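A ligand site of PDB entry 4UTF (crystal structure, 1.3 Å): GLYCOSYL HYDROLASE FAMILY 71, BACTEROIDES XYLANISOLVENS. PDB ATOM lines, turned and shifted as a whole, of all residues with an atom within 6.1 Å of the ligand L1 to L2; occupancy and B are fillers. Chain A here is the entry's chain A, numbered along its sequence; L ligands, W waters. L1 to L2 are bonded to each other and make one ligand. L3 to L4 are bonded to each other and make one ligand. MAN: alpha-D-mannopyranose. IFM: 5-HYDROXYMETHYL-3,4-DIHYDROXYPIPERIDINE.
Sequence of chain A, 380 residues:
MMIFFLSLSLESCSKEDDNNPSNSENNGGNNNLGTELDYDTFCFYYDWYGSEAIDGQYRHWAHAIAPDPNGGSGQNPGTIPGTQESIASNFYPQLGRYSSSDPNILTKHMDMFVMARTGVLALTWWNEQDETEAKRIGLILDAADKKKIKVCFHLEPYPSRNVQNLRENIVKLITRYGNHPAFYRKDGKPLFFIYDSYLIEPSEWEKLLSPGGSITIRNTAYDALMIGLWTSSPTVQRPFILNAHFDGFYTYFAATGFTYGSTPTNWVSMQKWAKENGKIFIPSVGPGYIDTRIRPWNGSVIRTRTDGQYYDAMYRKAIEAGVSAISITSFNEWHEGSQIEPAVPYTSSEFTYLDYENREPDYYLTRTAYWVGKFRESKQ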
ATOM      1  N   PHE A  44     -16.067  14.930  -1.193  1.00  0.00           N
ATOM      2  CA  PHE A  44     -15.235  14.325  -0.136  1.00  0.00           C
ATOM      3  C   PHE A  44     -14.147  15.282   0.335  1.00  0.00           C
ATOM      4  O   PHE A  44     -13.320  15.773  -0.449  1.00  0.00           O
ATOM      5  CB  PHE A  44     -14.641  13.006  -0.649  1.00  0.00           C
ATOM      6  CG  PHE A  44     -15.674  11.922  -0.823  1.00  0.00           C
ATOM      7  CD1 PHE A  44     -16.414  11.469   0.257  1.00  0.00           C
ATOM      8  CD2 PHE A  44     -15.957  11.378  -2.064  1.00  0.00           C
ATOM      9  CE1 PHE A  44     -17.397  10.527   0.112  1.00  0.00           C
ATOM     10  CE2 PHE A  44     -16.938  10.411  -2.213  1.00  0.00           C
ATOM     11  CZ  PHE A  44     -17.670   9.992  -1.132  1.00  0.00           C
ATOM     12  N   TYR A  46     -11.268  16.442   3.464  1.00  0.00           N
ATOM     13  CA  TYR A  46     -10.263  15.924   4.373  1.00  0.00           C
ATOM     14  C   TYR A  46      -9.829  17.046   5.302  1.00  0.00           C
ATOM     15  O   TYR A  46      -9.450  18.117   4.848  1.00  0.00           O
ATOM     16  CB  TYR A  46      -9.078  15.307   3.568  1.00  0.00           C
ATOM     17  CG  TYR A  46      -9.611  14.130   2.763  1.00  0.00           C
ATOM     18  CD1 TYR A  46     -10.222  14.305   1.523  1.00  0.00           C
ATOM     19  CD2 TYR A  46      -9.620  12.848   3.300  1.00  0.00           C
ATOM     20  CE1 TYR A  46     -10.824  13.253   0.864  1.00  0.00           C
ATOM     21  CE2 TYR A  46     -10.205  11.799   2.637  1.00  0.00           C
ATOM     22  CZ  TYR A  46     -10.814  11.997   1.413  1.00  0.00           C
ATOM     23  OH  TYR A  46     -11.432  10.973   0.754  1.00  0.00           O
ATOM     24  N   TRP A  48      -7.374  16.773   7.744  1.00  0.00           N
ATOM     25  CA  TRP A  48      -6.223  16.209   8.376  1.00  0.00           C
ATOM     26  C   TRP A  48      -4.917  17.039   8.200  1.00  0.00           C
ATOM     27  O   TRP A  48      -3.837  16.587   8.581  1.00  0.00           O
ATOM     28  CB  TRP A  48      -6.039  14.761   7.932  1.00  0.00           C
ATOM     29  CG  TRP A  48      -5.939  14.498   6.444  1.00  0.00           C
ATOM     30  CD1 TRP A  48      -5.432  15.314   5.472  1.00  0.00           C
ATOM     31  CD2 TRP A  48      -6.271  13.269   5.795  1.00  0.00           C
ATOM     32  NE1 TRP A  48      -5.452  14.675   4.255  1.00  0.00           N
ATOM     33  CE2 TRP A  48      -5.951  13.413   4.424  1.00  0.00           C
ATOM     34  CE3 TRP A  48      -6.790  12.041   6.236  1.00  0.00           C
ATOM     35  CZ2 TRP A  48      -6.124  12.389   3.508  1.00  0.00           C
ATOM     36  CZ3 TRP A  48      -6.973  11.025   5.309  1.00  0.00           C
ATOM     37  CH2 TRP A  48      -6.654  11.199   3.971  1.00  0.00           C
ATOM     38  N   HIS A  60       0.217  16.039   7.608  1.00  0.00           N
ATOM     39  CA  HIS A  60      -0.152  15.570   6.278  1.00  0.00           C
ATOM     40  C   HIS A  60       0.632  16.228   5.138  1.00  0.00           C
ATOM     41  O   HIS A  60       0.970  15.545   4.176  1.00  0.00           O
ATOM     42  CB  HIS A  60      -1.675  15.567   6.061  1.00  0.00           C
ATOM     43  CG  HIS A  60      -2.322  14.292   6.518  1.00  0.00           C
ATOM     44  ND1 HIS A  60      -2.699  13.317   5.623  1.00  0.00           N
ATOM     45  CD2 HIS A  60      -2.612  13.811   7.748  1.00  0.00           C
ATOM     46  CE1 HIS A  60      -3.211  12.296   6.286  1.00  0.00           C
ATOM     47  NE2 HIS A  60      -3.159  12.563   7.572  1.00  0.00           N
ATOM     48  N   HIS A  63       4.524  13.592   5.179  1.00  0.00           N
ATOM     49  CA  HIS A  63       3.892  12.268   5.054  1.00  0.00           C
ATOM     50  C   HIS A  63       4.915  11.204   4.723  1.00  0.00           C
ATOM     51  O   HIS A  63       5.835  11.441   3.922  1.00  0.00           O
ATOM     52  CB  HIS A  63       2.843  12.344   3.928  1.00  0.00           C
ATOM     53  CG  HIS A  63       1.747  11.318   3.959  1.00  0.00           C
ATOM     54  ND1 HIS A  63       1.928  10.000   3.614  1.00  0.00           N
ATOM     55  CD2 HIS A  63       0.420  11.466   4.188  1.00  0.00           C
ATOM     56  CE1 HIS A  63       0.765   9.369   3.667  1.00  0.00           C
ATOM     57  NE2 HIS A  63      -0.162  10.231   4.044  1.00  0.00           N
ATOM     58  N   THR A 124     -14.162  13.163   6.077  1.00  0.00           N
ATOM     59  CA  THR A 124     -13.383  12.004   6.513  1.00  0.00           C
ATOM     60  C   THR A 124     -13.454  11.903   8.035  1.00  0.00           C
ATOM     61  O   THR A 124     -13.374  12.901   8.738  1.00  0.00           O
ATOM     62  CB  THR A 124     -11.919  12.144   6.038  1.00  0.00           C
ATOM     63  OG1 THR A 124     -11.221  10.911   6.144  1.00  0.00           O
ATOM     64  CG2 THR A 124     -11.121  13.194   6.806  1.00  0.00           C
ATOM     65  N   TRP A 126     -12.074   9.399  11.278  1.00  0.00           N
ATOM     66  CA  TRP A 126     -11.097   8.378  11.638  1.00  0.00           C
ATOM     67  C   TRP A 126     -11.180   7.901  13.078  1.00  0.00           C
ATOM     68  O   TRP A 126     -10.353   7.081  13.509  1.00  0.00           O
ATOM     69  CB  TRP A 126      -9.674   8.904  11.331  1.00  0.00           C
ATOM     70  CG  TRP A 126      -9.384   8.934   9.856  1.00  0.00           C
ATOM     71  CD1 TRP A 126      -9.577   9.968   8.998  1.00  0.00           C
ATOM     72  CD2 TRP A 126      -8.937   7.824   9.048  1.00  0.00           C
ATOM     73  NE1 TRP A 126      -9.225   9.604   7.744  1.00  0.00           N
ATOM     74  CE2 TRP A 126      -8.836   8.293   7.727  1.00  0.00           C
ATOM     75  CE3 TRP A 126      -8.577   6.495   9.316  1.00  0.00           C
ATOM     76  CZ2 TRP A 126      -8.405   7.489   6.671  1.00  0.00           C
ATOM     77  CZ3 TRP A 126      -8.143   5.679   8.266  1.00  0.00           C
ATOM     78  CH2 TRP A 126      -8.073   6.185   6.956  1.00  0.00           C
ATOM     79  N   HIS A 154     -17.903  10.492   6.404  1.00  0.00           N
ATOM     80  CA  HIS A 154     -17.287   9.448   5.587  1.00  0.00           C
ATOM     81  C   HIS A 154     -16.502   8.559   6.559  1.00  0.00           C
ATOM     82  O   HIS A 154     -15.419   8.936   7.018  1.00  0.00           O
ATOM     83  CB  HIS A 154     -16.376  10.078   4.537  1.00  0.00           C
ATOM     84  CG  HIS A 154     -15.847   9.138   3.495  1.00  0.00           C
ATOM     85  ND1 HIS A 154     -14.856   9.514   2.614  1.00  0.00           N
ATOM     86  CD2 HIS A 154     -16.214   7.880   3.145  1.00  0.00           C
ATOM     87  CE1 HIS A 154     -14.619   8.520   1.768  1.00  0.00           C
ATOM     88  NE2 HIS A 154     -15.438   7.528   2.060  1.00  0.00           N
ATOM     89  N   GLU A 156     -14.203   6.021   7.914  1.00  0.00           N
ATOM     90  CA  GLU A 156     -12.967   5.432   7.421  1.00  0.00           C
ATOM     91  C   GLU A 156     -12.633   4.106   8.129  1.00  0.00           C
ATOM     92  O   GLU A 156     -13.271   3.803   9.136  1.00  0.00           O
ATOM     93  CB  GLU A 156     -11.837   6.446   7.564  1.00  0.00           C
ATOM     94  CG  GLU A 156     -12.081   7.723   6.785  1.00  0.00           C
ATOM     95  CD  GLU A 156     -11.672   7.646   5.328  1.00  0.00           C
ATOM     96  OE1 GLU A 156     -11.364   6.550   4.830  1.00  0.00           O
ATOM     97  OE2 GLU A 156     -11.667   8.729   4.679  1.00  0.00           O
ATOM     98  N   PRO A 157     -11.651   3.354   7.593  1.00  0.00           N
ATOM     99  CA  PRO A 157     -11.318   2.061   8.194  1.00  0.00           C
ATOM    100  C   PRO A 157     -10.411   2.224   9.422  1.00  0.00           C
ATOM    101  O   PRO A 157      -9.202   1.946   9.374  1.00  0.00           O
ATOM    102  CB  PRO A 157     -10.682   1.269   7.056  1.00  0.00           C
ATOM    103  CG  PRO A 157     -10.739   2.136   5.847  1.00  0.00           C
ATOM    104  CD  PRO A 157     -10.988   3.528   6.289  1.00  0.00           C
ATOM    105  N   TYR A 195     -16.230   3.763   3.880  1.00  0.00           N
ATOM    106  CA  TYR A 195     -15.097   3.439   3.033  1.00  0.00           C
ATOM    107  C   TYR A 195     -14.620   2.012   3.284  1.00  0.00           C
ATOM    108  O   TYR A 195     -14.608   1.554   4.444  1.00  0.00           O
ATOM    109  CB  TYR A 195     -13.960   4.457   3.182  1.00  0.00           C
ATOM    110  CG  TYR A 195     -12.871   4.225   2.134  1.00  0.00           C
ATOM    111  CD1 TYR A 195     -13.120   4.405   0.785  1.00  0.00           C
ATOM    112  CD2 TYR A 195     -11.632   3.734   2.507  1.00  0.00           C
ATOM    113  CE1 TYR A 195     -12.161   4.132  -0.181  1.00  0.00           C
ATOM    114  CE2 TYR A 195     -10.670   3.448   1.547  1.00  0.00           C
ATOM    115  CZ  TYR A 195     -10.959   3.620   0.200  1.00  0.00           C
ATOM    116  OH  TYR A 195     -10.001   3.328  -0.752  1.00  0.00           O
ATOM    117  N   TYR A 250     -21.604   3.725  -3.368  1.00  0.00           N
ATOM    118  CA  TYR A 250     -20.774   4.700  -4.053  1.00  0.00           C
ATOM    119  C   TYR A 250     -19.518   4.005  -4.545  1.00  0.00           C
ATOM    120  O   TYR A 250     -19.295   2.863  -4.211  1.00  0.00           O
ATOM    121  CB  TYR A 250     -20.450   5.914  -3.160  1.00  0.00           C
ATOM    122  CG  TYR A 250     -19.403   5.726  -2.072  1.00  0.00           C
ATOM    123  CD1 TYR A 250     -19.535   4.767  -1.085  1.00  0.00           C
ATOM    124  CD2 TYR A 250     -18.298   6.575  -1.988  1.00  0.00           C
ATOM    125  CE1 TYR A 250     -18.608   4.622  -0.072  1.00  0.00           C
ATOM    126  CE2 TYR A 250     -17.360   6.451  -0.969  1.00  0.00           C
ATOM    127  CZ  TYR A 250     -17.524   5.470   0.002  1.00  0.00           C
ATOM    128  OH  TYR A 250     -16.617   5.317   1.027  1.00  0.00           O
ATOM    129  N   TYR A 252     -16.201   5.828  -5.084  1.00  0.00           N
ATOM    130  CA  TYR A 252     -15.046   6.608  -4.601  1.00  0.00           C
ATOM    131  C   TYR A 252     -13.943   6.949  -5.625  1.00  0.00           C
ATOM    132  O   TYR A 252     -13.632   8.114  -5.826  1.00  0.00           O
ATOM    133  CB  TYR A 252     -14.369   6.018  -3.319  1.00  0.00           C
ATOM    134  CG  TYR A 252     -13.397   7.049  -2.795  1.00  0.00           C
ATOM    135  CD1 TYR A 252     -13.832   8.177  -2.100  1.00  0.00           C
ATOM    136  CD2 TYR A 252     -12.049   6.951  -3.085  1.00  0.00           C
ATOM    137  CE1 TYR A 252     -12.975   9.186  -1.732  1.00  0.00           C
ATOM    138  CE2 TYR A 252     -11.178   7.975  -2.727  1.00  0.00           C
ATOM    139  CZ  TYR A 252     -11.637   9.085  -2.040  1.00  0.00           C
ATOM    140  OH  TYR A 252     -10.744  10.105  -1.740  1.00  0.00           O
ATOM    141  N   ILE A 294       3.769  10.251  -2.747  1.00  0.00           N
ATOM    142  CA  ILE A 294       3.663   9.347  -1.608  1.00  0.00           C
ATOM    143  C   ILE A 294       3.670   7.863  -1.988  1.00  0.00           C
ATOM    144  O   ILE A 294       3.964   7.036  -1.124  1.00  0.00           O
ATOM    145  CB  ILE A 294       2.484   9.638  -0.650  1.00  0.00           C
ATOM    146  CG1 ILE A 294       1.121   9.560  -1.362  1.00  0.00           C
ATOM    147  CG2 ILE A 294       2.666  10.986   0.028  1.00  0.00           C
ATOM    148  CD1 ILE A 294       0.019   9.120  -0.406  1.00  0.00           C
ATOM    149  N   ARG A 295       3.381   7.522  -3.247  1.00  0.00           N
ATOM    150  CA  ARG A 295       3.359   6.125  -3.722  1.00  0.00           C
ATOM    151  C   ARG A 295       4.079   6.060  -5.061  1.00  0.00           C
ATOM    152  O   ARG A 295       3.437   5.948  -6.112  1.00  0.00           O
ATOM    153  CB  ARG A 295       1.919   5.583  -3.845  1.00  0.00           C
ATOM    154  CG  ARG A 295       1.104   5.773  -2.565  1.00  0.00           C
ATOM    155  CD  ARG A 295      -0.209   5.026  -2.592  1.00  0.00           C
ATOM    156  NE  ARG A 295      -1.037   5.293  -1.420  1.00  0.00           N
ATOM    157  CZ  ARG A 295      -2.108   6.084  -1.386  1.00  0.00           C
ATOM    158  NH1 ARG A 295      -2.535   6.717  -2.466  1.00  0.00           N
ATOM    159  NH2 ARG A 295      -2.772   6.283  -0.240  1.00  0.00           N
ATOM    160  N   GLU A 333      -8.175  15.822  -1.350  1.00  0.00           N
ATOM    161  CA  GLU A 333      -7.246  14.703  -1.155  1.00  0.00           C
ATOM    162  C   GLU A 333      -5.996  15.034  -2.005  1.00  0.00           C
ATOM    163  O   GLU A 333      -5.822  14.591  -3.145  1.00  0.00           O
ATOM    164  CB  GLU A 333      -7.861  13.338  -1.492  1.00  0.00           C
ATOM    165  CG  GLU A 333      -7.514  12.199  -0.523  1.00  0.00           C
ATOM    166  CD  GLU A 333      -6.048  11.850  -0.417  1.00  0.00           C
ATOM    167  OE1 GLU A 333      -5.182  12.649  -0.833  1.00  0.00           O
ATOM    168  OE2 GLU A 333      -5.763  10.764   0.163  1.00  0.00           O
ATOM    169  N   HIS A 335      -2.913  14.299  -1.522  1.00  0.00           N
ATOM    170  CA  HIS A 335      -1.953  13.223  -1.683  1.00  0.00           C
ATOM    171  C   HIS A 335      -2.211  12.441  -2.960  1.00  0.00           C
ATOM    172  O   HIS A 335      -1.295  11.897  -3.563  1.00  0.00           O
ATOM    173  CB  HIS A 335      -1.989  12.230  -0.498  1.00  0.00           C
ATOM    174  CG  HIS A 335      -1.833  12.899   0.825  1.00  0.00           C
ATOM    175  ND1 HIS A 335      -2.715  12.801   1.892  1.00  0.00           N
ATOM    176  CD2 HIS A 335      -0.890  13.786   1.211  1.00  0.00           C
ATOM    177  CE1 HIS A 335      -2.265  13.549   2.895  1.00  0.00           C
ATOM    178  NE2 HIS A 335      -1.173  14.175   2.486  1.00  0.00           N
ATOM    179  N   GLU A 336      -3.491  12.342  -3.329  1.00  0.00           N
ATOM    180  CA  GLU A 336      -3.939  11.537  -4.447  1.00  0.00           C
ATOM    181  C   GLU A 336      -4.223  12.347  -5.704  1.00  0.00           C
ATOM    182  O   GLU A 336      -4.543  11.777  -6.747  1.00  0.00           O
ATOM    183  CB  GLU A 336      -5.117  10.670  -4.021  1.00  0.00           C
ATOM    184  CG  GLU A 336      -4.685   9.616  -3.008  1.00  0.00           C
ATOM    185  CD  GLU A 336      -5.736   8.618  -2.590  1.00  0.00           C
ATOM    186  OE1 GLU A 336      -6.957   8.908  -2.706  1.00  0.00           O
ATOM    187  OE2 GLU A 336      -5.314   7.519  -2.114  1.00  0.00           O
HETATM  188  C1  MAN L   1      -5.205   6.583   3.331  1.00  0.00           C
HETATM  189  C2  MAN L   1      -4.674   6.565   4.760  1.00  0.00           C
HETATM  190  C3  MAN L   1      -4.203   7.951   5.203  1.00  0.00           C
HETATM  191  C4  MAN L   1      -3.204   8.524   4.190  1.00  0.00           C
HETATM  192  C5  MAN L   1      -3.892   8.501   2.806  1.00  0.00           C
HETATM  193  C6  MAN L   1      -2.957   9.009   1.695  1.00  0.00           C
HETATM  194  O2  MAN L   1      -3.598   5.641   4.779  1.00  0.00           O
HETATM  195  O3  MAN L   1      -3.587   7.897   6.504  1.00  0.00           O
HETATM  196  O4  MAN L   1      -2.870   9.861   4.540  1.00  0.00           O
HETATM  197  O5  MAN L   1      -4.248   7.169   2.462  1.00  0.00           O
HETATM  198  O6  MAN L   1      -3.612   9.071   0.434  1.00  0.00           O
HETATM  199  O4  IFM L   2      -9.096   6.184   3.497  1.00  0.00           O
HETATM  200  C4  IFM L   2      -8.729   7.223   2.552  1.00  0.00           C
HETATM  201  C3  IFM L   2      -7.267   7.035   2.173  1.00  0.00           C
HETATM  202  O3  IFM L   2      -6.475   7.244   3.369  1.00  0.00           O
HETATM  203  C2  IFM L   2      -6.773   7.998   1.077  1.00  0.00           C
HETATM  204  N   IFM L   2      -7.702   7.921  -0.050  1.00  0.00           N
HETATM  205  C1  IFM L   2      -9.100   8.232   0.286  1.00  0.00           C
HETATM  206  C5  IFM L   2      -9.605   7.189   1.297  1.00  0.00           C
HETATM  207  C6  IFM L   2     -11.104   7.442   1.588  1.00  0.00           C
HETATM  208  O6  IFM L   2     -11.334   8.750   2.135  1.00  0.00           O
HETATM  209  C1  MAN L   3      -6.478  -0.636  -2.577  1.00  0.00           C
HETATM  210  C2  MAN L   3      -6.849   0.427  -1.537  1.00  0.00           C
HETATM  211  C3  MAN L   3      -8.188   0.140  -0.902  1.00  0.00           C
HETATM  212  C4  MAN L   3      -9.242  -0.068  -1.993  1.00  0.00           C
HETATM  213  C5  MAN L   3      -8.780  -1.094  -3.032  1.00  0.00           C
HETATM  214  C6  MAN L   3      -9.772  -1.244  -4.185  1.00  0.00           C
HETATM  215  O1  MAN L   3      -6.212  -1.867  -1.925  1.00  0.00           O
HETATM  216  O2  MAN L   3      -6.933   1.692  -2.191  1.00  0.00           O
HETATM  217  O3  MAN L   3      -8.562   1.165   0.033  1.00  0.00           O
HETATM  218  O4  MAN L   3     -10.477  -0.520  -1.450  1.00  0.00           O
HETATM  219  O5  MAN L   3      -7.509  -0.745  -3.578  1.00  0.00           O
HETATM  220  O6  MAN L   3      -9.448  -2.337  -4.996  1.00  0.00           O
HETATM  221  C1  MAN L   4      -5.833   2.580  -1.941  1.00  0.00           C
HETATM  222  C2  MAN L   4      -6.148   3.884  -2.656  1.00  0.00           C
HETATM  223  C3  MAN L   4      -5.947   3.811  -4.175  1.00  0.00           C
HETATM  224  C4  MAN L   4      -4.518   3.387  -4.536  1.00  0.00           C
HETATM  225  C5  MAN L   4      -4.266   2.074  -3.791  1.00  0.00           C
HETATM  226  C6  MAN L   4      -2.796   1.705  -3.916  1.00  0.00           C
HETATM  227  O2  MAN L   4      -5.241   4.806  -2.132  1.00  0.00           O
HETATM  228  O3  MAN L   4      -6.257   5.047  -4.831  1.00  0.00           O
HETATM  229  O4  MAN L   4      -4.315   3.216  -5.954  1.00  0.00           O
HETATM  230  O5  MAN L   4      -4.558   2.171  -2.385  1.00  0.00           O
HETATM  231  O6  MAN L   4      -2.612   0.368  -3.500  1.00  0.00           O
HETATM  232  O   HOH W   1      -4.371   4.984   7.816  1.00  0.00           O
HETATM  233  O   HOH W   2      -7.707   3.849   4.002  1.00  0.00           O
HETATM  234  O   HOH W   3      -8.630   5.729  -1.411  1.00  0.00           O
HETATM  235  O   HOH W   4      -4.926   4.162   0.848  1.00  0.00           O
HETATM  236  O   HOH W   5      -2.273   4.813   2.385  1.00  0.00           O
HETATM  237  O   HOH W   6      -1.002   6.305   6.597  1.00  0.00           O
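His 60 touches the ligand L1 to L2. Trp 126 touches the ligand L1 to L2. CE1 of His 154 touches O6 of IFM L2, 3.3 Å away. Tyr 195 touches the ligand L1 to L2. OH of Tyr 252 touches C1 of IFM L2, at 3.2 Å. Ile 294 touches the ligand L1 to L2. CB of His 335 touches O6 of MAN L1 (3.7 Å). Hydrophobic or aromatic side chains within 4 Å of the ligand L1 to L2: Tyr 46, His 60, His 63, Trp 126, His 154, Tyr 195, Tyr 252, Ile 294 and His 335.
Water W3 lies within hydrogen-bond range of a nitrogen (N) of IFM L2 (2.7 Å) and the side-chain hydroxyl of Tyr 195 (2.8 Å). Water W5 bridges O2 of MAN L1 (2.9 Å) and NH2 of Arg 295 (3.0 Å). Water W4 lies within hydrogen-bond range of an oxygen (O2) of MAN L4, the guanidinium group (NH2) of Arg 295 and an oxygen (O5) of MAN L1.
The side-chain carboxylate (OE2) of Glu 156 is in hydrogen-bond range of the side-chain hydroxyl (OG1) of Thr 124 (2.7 Å). The side-chain carboxylate (OE1) of Glu 333 lies within hydrogen-bond range of the backbone NH (N) of Glu 336 (3.0 Å). OE1 of Glu 333 lies within hydrogen-bond range of N of His 335. The side-chain carboxylate (OE2) of Glu 336 is in salt-bridge range of the guanidinium group (NH1) of Arg 295 (2.9 Å). ND1 of His 60 lies within hydrogen-bond range of NE1 of Trp 48, 3.4 Å away. NE2 of His 154 sits at hydrogen-bond distance from OH of Tyr 250 (2.7 Å). The indole nitrogen (NE1) of Trp 126 lies within hydrogen-bond range of the side-chain hydroxyl (OG1) of Thr 124 (2.9 Å). N of Tyr 195 sits close to OH of Tyr 250 (3.3 Å).
The side-chain carboxylate (OE2) of Glu 156 lies within hydrogen-bond range of an oxygen (O6) of IFM L2 (2.6 Å). The side-chain hydroxyl of Tyr 46 is in hydrogen-bond range of an oxygen (O6) of IFM L2 (2.6 Å). N of IFM L2 is in salt-bridge range of OE2 of Glu 333, at 3.4 Å. O4 of MAN L1 sits at hydrogen-bond distance from NE2 of His 63, 2.8 Å away. A nitrogen (N) of IFM L2 is in salt-bridge range of the side-chain carboxylate of Glu 336 (2.9 Å). The guanidinium group (NH2) of Arg 295 lies within hydrogen-bond range of an oxygen (O6) of MAN L1 (3.0 Å). OE2 of Glu 336 is in hydrogen-bond range of O2 of MAN L4, 2.7 Å away. The guanidinium group (NH1) of Arg 295 is in hydrogen-bond range of an oxygen (O2) of MAN L4 (3.3 Å). The side-chain hydroxyl of Tyr 195 lies within hydrogen-bond range of an oxygen (O3) of MAN L3.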
